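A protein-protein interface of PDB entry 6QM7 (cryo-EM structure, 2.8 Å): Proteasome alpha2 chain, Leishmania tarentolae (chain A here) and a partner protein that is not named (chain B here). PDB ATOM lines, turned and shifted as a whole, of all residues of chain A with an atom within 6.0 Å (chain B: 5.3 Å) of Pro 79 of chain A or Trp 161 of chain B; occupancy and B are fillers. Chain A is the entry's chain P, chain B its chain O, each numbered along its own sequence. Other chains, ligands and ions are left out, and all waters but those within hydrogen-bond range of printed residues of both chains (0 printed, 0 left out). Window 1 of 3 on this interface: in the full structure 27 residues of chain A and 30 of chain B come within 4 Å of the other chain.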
ATOM      1  N   PRO A  51      16.633   8.761   8.259  1.00  0.00           N
ATOM      2  CA  PRO A  51      17.114  10.045   8.781  1.00  0.00           C
ATOM      3  C   PRO A  51      18.641  10.194   8.692  1.00  0.00           C
ATOM      4  O   PRO A  51      19.093  11.190   8.160  1.00  0.00           O
ATOM      5  CB  PRO A  51      16.653  10.036  10.249  1.00  0.00           C
ATOM      6  CG  PRO A  51      15.421   9.143  10.260  1.00  0.00           C
ATOM      7  CD  PRO A  51      15.628   8.141   9.140  1.00  0.00           C
ATOM      8  N   VAL A  55      20.849   4.518  11.246  1.00  0.00           N
ATOM      9  CA  VAL A  55      19.619   3.683  11.339  1.00  0.00           C
ATOM     10  C   VAL A  55      19.911   2.351  10.656  1.00  0.00           C
ATOM     11  O   VAL A  55      20.442   2.375   9.532  1.00  0.00           O
ATOM     12  CB  VAL A  55      18.394   4.387  10.730  1.00  0.00           C
ATOM     13  CG1 VAL A  55      17.141   3.537  10.852  1.00  0.00           C
ATOM     14  CG2 VAL A  55      18.174   5.752  11.370  1.00  0.00           C
ATOM     15  N   ILE A  60      13.906  -0.692   9.085  1.00  0.00           N
ATOM     16  CA  ILE A  60      12.888   0.143   8.387  1.00  0.00           C
ATOM     17  C   ILE A  60      12.137  -0.786   7.438  1.00  0.00           C
ATOM     18  O   ILE A  60      12.769  -1.650   6.804  1.00  0.00           O
ATOM     19  CB  ILE A  60      13.474   1.341   7.622  1.00  0.00           C
ATOM     20  CG1 ILE A  60      14.401   2.204   8.482  1.00  0.00           C
ATOM     21  CG2 ILE A  60      12.347   2.169   7.014  1.00  0.00           C
ATOM     22  CD1 ILE A  60      15.328   3.098   7.663  1.00  0.00           C
ATOM     23  N   TYR A  74       3.007   2.272   1.776  1.00  0.00           N
ATOM     24  CA  TYR A  74       2.269   3.408   2.347  1.00  0.00           C
ATOM     25  C   TYR A  74       3.079   4.681   2.191  1.00  0.00           C
ATOM     26  O   TYR A  74       4.300   4.642   1.980  1.00  0.00           O
ATOM     27  CB  TYR A  74       1.995   3.163   3.828  1.00  0.00           C
ATOM     28  CG  TYR A  74       3.169   3.437   4.739  1.00  0.00           C
ATOM     29  CD1 TYR A  74       3.407   4.705   5.243  1.00  0.00           C
ATOM     30  CD2 TYR A  74       4.056   2.436   5.084  1.00  0.00           C
ATOM     31  CE1 TYR A  74       4.507   4.978   6.043  1.00  0.00           C
ATOM     32  CE2 TYR A  74       5.151   2.688   5.897  1.00  0.00           C
ATOM     33  CZ  TYR A  74       5.385   3.964   6.373  1.00  0.00           C
ATOM     34  OH  TYR A  74       6.461   4.218   7.178  1.00  0.00           O
ATOM     35  N   GLY A  76       3.040   8.729   4.278  1.00  0.00           N
ATOM     36  CA  GLY A  76       2.513   9.581   5.352  1.00  0.00           C
ATOM     37  C   GLY A  76       2.965   9.056   6.683  1.00  0.00           C
ATOM     38  O   GLY A  76       4.118   8.612   6.783  1.00  0.00           O
ATOM     39  N   MET A  77       2.075   9.068   7.659  1.00  0.00           N
ATOM     40  CA  MET A  77       2.420   8.736   9.056  1.00  0.00           C
ATOM     41  C   MET A  77       2.624   7.223   9.166  1.00  0.00           C
ATOM     42  O   MET A  77       1.640   6.463   9.119  1.00  0.00           O
ATOM     43  CB  MET A  77       1.326   9.228   9.995  1.00  0.00           C
ATOM     44  CG  MET A  77       1.056  10.698   9.810  1.00  0.00           C
ATOM     45  SD  MET A  77       0.234  11.410  11.237  1.00  0.00           S
ATOM     46  CE  MET A  77       1.092  12.988  11.233  1.00  0.00           C
ATOM     47  N   GLY A  78       3.887   6.813   9.239  1.00  0.00           N
ATOM     48  CA  GLY A  78       4.273   5.410   9.443  1.00  0.00           C
ATOM     49  C   GLY A  78       3.439   4.770  10.538  1.00  0.00           C
ATOM     50  O   GLY A  78       2.771   3.770  10.294  1.00  0.00           O
ATOM     51  N   PRO A  79       3.454   5.339  11.760  1.00  0.00           N
ATOM     52  CA  PRO A  79       2.799   4.722  12.914  1.00  0.00           C
ATOM     53  C   PRO A  79       1.298   4.482  12.732  1.00  0.00           C
ATOM     54  O   PRO A  79       0.815   3.515  13.273  1.00  0.00           O
ATOM     55  CB  PRO A  79       3.014   5.752  14.027  1.00  0.00           C
ATOM     56  CG  PRO A  79       4.267   6.491  13.601  1.00  0.00           C
ATOM     57  CD  PRO A  79       4.133   6.595  12.102  1.00  0.00           C
ATOM     58  N   ASP A  80       0.616   5.385  12.026  1.00  0.00           N
ATOM     59  CA  ASP A  80      -0.806   5.250  11.617  1.00  0.00           C
ATOM     60  C   ASP A  80      -0.964   4.024  10.724  1.00  0.00           C
ATOM     61  O   ASP A  80      -1.858   3.224  11.002  1.00  0.00           O
ATOM     62  CB  ASP A  80      -1.293   6.471  10.842  1.00  0.00           C
ATOM     63  CG  ASP A  80      -1.500   7.695  11.704  1.00  0.00           C
ATOM     64  OD1 ASP A  80      -0.944   7.734  12.816  1.00  0.00           O
ATOM     65  OD2 ASP A  80      -2.219   8.615  11.248  1.00  0.00           O
ATOM     66  N   CYS A  81      -0.139   3.901   9.685  1.00  0.00           N
ATOM     67  CA  CYS A  81      -0.161   2.742   8.761  1.00  0.00           C
ATOM     68  C   CYS A  81      -0.015   1.447   9.531  1.00  0.00           C
ATOM     69  O   CYS A  81      -0.712   0.479   9.180  1.00  0.00           O
ATOM     70  CB  CYS A  81       0.953   2.787   7.738  1.00  0.00           C
ATOM     71  SG  CYS A  81       0.350   3.602   6.249  1.00  0.00           S
ATOM     72  N   ARG A  82       0.858   1.428  10.530  1.00  0.00           N
ATOM     73  CA  ARG A  82       1.102   0.190  11.290  1.00  0.00           C
ATOM     74  C   ARG A  82      -0.243  -0.277  11.863  1.00  0.00           C
ATOM     75  O   ARG A  82      -0.448  -1.501  11.900  1.00  0.00           O
ATOM     76  CB  ARG A  82       2.241   0.349  12.306  1.00  0.00           C
ATOM     77  CG  ARG A  82       2.890  -0.969  12.730  1.00  0.00           C
ATOM     78  CD  ARG A  82       2.791  -2.110  11.700  1.00  0.00           C
ATOM     79  NE  ARG A  82       3.327  -3.407  12.108  1.00  0.00           N
ATOM     80  CZ  ARG A  82       4.601  -3.788  12.026  1.00  0.00           C
ATOM     81  NH1 ARG A  82       5.527  -2.963  11.555  1.00  0.00           N
ATOM     82  NH2 ARG A  82       4.947  -5.000  12.439  1.00  0.00           N
ATOM     83  N   VAL A  83      -1.154   0.640  12.206  1.00  0.00           N
ATOM     84  CA  VAL A  83      -2.520   0.320  12.711  1.00  0.00           C
ATOM     85  C   VAL A  83      -3.337  -0.361  11.612  1.00  0.00           C
ATOM     86  O   VAL A  83      -3.984  -1.388  11.911  1.00  0.00           O
ATOM     87  CB  VAL A  83      -3.246   1.579  13.216  1.00  0.00           C
ATOM     88  CG1 VAL A  83      -4.707   1.318  13.559  1.00  0.00           C
ATOM     89  CG2 VAL A  83      -2.507   2.181  14.397  1.00  0.00           C
ATOM     90  N   GLY B 116       5.406   1.358  20.156  1.00  0.00           N
ATOM     91  CA  GLY B 116       5.039   2.283  19.073  1.00  0.00           C
ATOM     92  C   GLY B 116       3.543   2.330  18.867  1.00  0.00           C
ATOM     93  O   GLY B 116       3.024   3.419  18.636  1.00  0.00           O
ATOM     94  N   ASP B 117       2.882   1.180  18.922  1.00  0.00           N
ATOM     95  CA  ASP B 117       1.411   1.072  18.749  1.00  0.00           C
ATOM     96  C   ASP B 117       0.724   1.812  19.885  1.00  0.00           C
ATOM     97  O   ASP B 117      -0.286   2.461  19.620  1.00  0.00           O
ATOM     98  CB  ASP B 117       0.921  -0.377  18.750  1.00  0.00           C
ATOM     99  CG  ASP B 117       1.081  -1.151  17.443  1.00  0.00           C
ATOM    100  OD1 ASP B 117       1.196  -0.517  16.341  1.00  0.00           O
ATOM    101  OD2 ASP B 117       1.055  -2.407  17.535  1.00  0.00           O
ATOM    102  N   GLN B 120       1.166   5.531  19.312  1.00  0.00           N
ATOM    103  CA  GLN B 120       0.321   5.971  18.178  1.00  0.00           C
ATOM    104  C   GLN B 120      -1.091   6.201  18.679  1.00  0.00           C
ATOM    105  O   GLN B 120      -1.661   7.230  18.317  1.00  0.00           O
ATOM    106  CB  GLN B 120       0.268   4.997  17.008  1.00  0.00           C
ATOM    107  CG  GLN B 120      -0.440   5.580  15.780  1.00  0.00           C
ATOM    108  CD  GLN B 120      -1.934   5.353  15.713  1.00  0.00           C
ATOM    109  OE1 GLN B 120      -2.520   4.608  16.500  1.00  0.00           O
ATOM    110  NE2 GLN B 120      -2.572   6.003  14.749  1.00  0.00           N
ATOM    111  N   THR B 155      14.593   2.315  19.152  1.00  0.00           N
ATOM    112  CA  THR B 155      13.950   3.532  19.702  1.00  0.00           C
ATOM    113  C   THR B 155      12.476   3.544  19.348  1.00  0.00           C
ATOM    114  O   THR B 155      12.129   3.081  18.280  1.00  0.00           O
ATOM    115  CB  THR B 155      14.537   4.836  19.163  1.00  0.00           C
ATOM    116  OG1 THR B 155      14.367   4.862  17.744  1.00  0.00           O
ATOM    117  CG2 THR B 155      15.990   4.997  19.554  1.00  0.00           C
ATOM    118  N   VAL B 156      11.673   4.063  20.261  1.00  0.00           N
ATOM    119  CA  VAL B 156      10.251   4.434  20.059  1.00  0.00           C
ATOM    120  C   VAL B 156      10.128   5.884  20.477  1.00  0.00           C
ATOM    121  O   VAL B 156      10.548   6.188  21.607  1.00  0.00           O
ATOM    122  CB  VAL B 156       9.321   3.563  20.906  1.00  0.00           C
ATOM    123  CG1 VAL B 156       7.865   3.805  20.550  1.00  0.00           C
ATOM    124  CG2 VAL B 156       9.678   2.100  20.761  1.00  0.00           C
ATOM    125  N   ASP B 157       9.584   6.728  19.616  1.00  0.00           N
ATOM    126  CA  ASP B 157       9.411   8.165  19.931  1.00  0.00           C
ATOM    127  C   ASP B 157       7.936   8.425  20.232  1.00  0.00           C
ATOM    128  O   ASP B 157       7.106   7.533  20.083  1.00  0.00           O
ATOM    129  CB  ASP B 157      10.035   9.011  18.830  1.00  0.00           C
ATOM    130  CG  ASP B 157       9.409   8.822  17.461  1.00  0.00           C
ATOM    131  OD1 ASP B 157      10.175   8.899  16.466  1.00  0.00           O
ATOM    132  OD2 ASP B 157       8.170   8.637  17.383  1.00  0.00           O
ATOM    133  N   ALA B 159       5.603   9.974  18.624  1.00  0.00           N
ATOM    134  CA  ALA B 159       4.749   9.844  17.421  1.00  0.00           C
ATOM    135  C   ALA B 159       4.264   8.400  17.272  1.00  0.00           C
ATOM    136  O   ALA B 159       3.195   8.210  16.638  1.00  0.00           O
ATOM    137  CB  ALA B 159       5.499  10.273  16.183  1.00  0.00           C
ATOM    138  N   GLY B 160       5.019   7.448  17.833  1.00  0.00           N
ATOM    139  CA  GLY B 160       4.838   5.996  17.666  1.00  0.00           C
ATOM    140  C   GLY B 160       5.884   5.416  16.729  1.00  0.00           C
ATOM    141  O   GLY B 160       5.866   4.176  16.509  1.00  0.00           O
ATOM    142  N   TRP B 161       6.757   6.264  16.172  1.00  0.00           N
ATOM    143  CA  TRP B 161       7.730   5.834  15.142  1.00  0.00           C
ATOM    144  C   TRP B 161       8.796   4.981  15.821  1.00  0.00           C
ATOM    145  O   TRP B 161       9.473   5.478  16.724  1.00  0.00           O
ATOM    146  CB  TRP B 161       8.324   7.006  14.351  1.00  0.00           C
ATOM    147  CG  TRP B 161       9.139   6.524  13.188  1.00  0.00           C
ATOM    148  CD1 TRP B 161       8.695   6.214  11.931  1.00  0.00           C
ATOM    149  CD2 TRP B 161      10.544   6.212  13.209  1.00  0.00           C
ATOM    150  NE1 TRP B 161       9.732   5.755  11.162  1.00  0.00           N
ATOM    151  CE2 TRP B 161      10.880   5.747  11.917  1.00  0.00           C
ATOM    152  CE3 TRP B 161      11.551   6.295  14.185  1.00  0.00           C
ATOM    153  CZ2 TRP B 161      12.187   5.374  11.583  1.00  0.00           C
ATOM    154  CZ3 TRP B 161      12.840   5.925  13.854  1.00  0.00           C
ATOM    155  CH2 TRP B 161      13.152   5.470  12.568  1.00  0.00           C
ATOM    156  N   THR B 162       8.894   3.726  15.399  1.00  0.00           N
ATOM    157  CA  THR B 162       9.796   2.683  15.948  1.00  0.00           C
ATOM    158  C   THR B 162      10.874   2.400  14.908  1.00  0.00           C
ATOM    159  O   THR B 162      10.531   2.299  13.729  1.00  0.00           O
ATOM    160  CB  THR B 162       9.001   1.417  16.289  1.00  0.00           C
ATOM    161  OG1 THR B 162       7.998   1.740  17.249  1.00  0.00           O
ATOM    162  CG2 THR B 162       9.859   0.304  16.838  1.00  0.00           C
ATOM    163  N   GLY B 163      12.121   2.294  15.342  1.00  0.00           N
ATOM    164  CA  GLY B 163      13.280   2.115  14.457  1.00  0.00           C
ATOM    165  C   GLY B 163      14.388   1.337  15.135  1.00  0.00           C
ATOM    166  O   GLY B 163      14.660   1.586  16.316  1.00  0.00           O
ATOM    167  N   HIS B 165      18.506   0.703  15.205  1.00  0.00           N
ATOM    168  CA  HIS B 165      19.657   1.628  15.084  1.00  0.00           C
ATOM    169  C   HIS B 165      20.951   0.843  15.192  1.00  0.00           C
ATOM    170  O   HIS B 165      20.951  -0.209  15.847  1.00  0.00           O
ATOM    171  CB  HIS B 165      19.598   2.730  16.140  1.00  0.00           C
ATOM    172  CG  HIS B 165      18.414   3.605  15.978  1.00  0.00           C
ATOM    173  ND1 HIS B 165      18.429   4.711  15.164  1.00  0.00           N
ATOM    174  CD2 HIS B 165      17.179   3.521  16.510  1.00  0.00           C
ATOM    175  CE1 HIS B 165      17.241   5.287  15.208  1.00  0.00           C
ATOM    176  NE2 HIS B 165      16.454   4.576  16.029  1.00  0.00           N
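Printed residues of chain A that touch a printed residue of chain B: Val 55, Pro 79, Asp 80 and Val 83.
OG1 of Thr 155 of chain B lies within hydrogen-bond range of NE2 of His 165 of chain B (2.7 Å). OD2 of Asp 157 of chain B is in hydrogen-bond range of N of Ala 159 of chain B (3.1 Å). The side-chain carboxylate (OD2) of Asp 157 of chain B lies within hydrogen-bond range of the backbone NH (N) of Gly 160 of chain B. The side-chain carboxylate (OD2) of Asp 157 of chain B sits at hydrogen-bond distance from the backbone NH (N) of Trp 161 of chain B, 3.0 Å away. O of Gly 160 of chain B lies within hydrogen-bond range of OG1 of Thr 162 of chain B, 3.3 Å away. O of Gly 163 of chain B sits close to NE2 of His 165 of chain B.
The side-chain carboxylate (OD1) of Asp 80 of chain A is in hydrogen-bond range of the side-chain amide nitrogen (NE2) of Gln 120 of chain B, at 3.1 Å.
Pro 79 of chain A touches just these residues of chain B: Gln 120, Ala 159, Gly 160 and Trp 161. Trp 161 of chain B touches one residue of chain A. Printed residues of chain A within 4 Å of His 165 of chain B: Val 55 (3.9 Å). Of the printed residues of chain A, Gly 160 of chain B touches Pro 79.
Among the printed residues, merely in contact across the chains: Val 55 of chain A with His 165 of chain B, Pro 79 of chain A with Gln 120 of chain B, Pro 79 of chain A with Ala 159 of chain B, Pro 79 of chain A with Gly 160 of chain B, Pro 79 of chain A with Trp 161 of chain B and Val 83 of chain A with Gln 120 of chain B.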
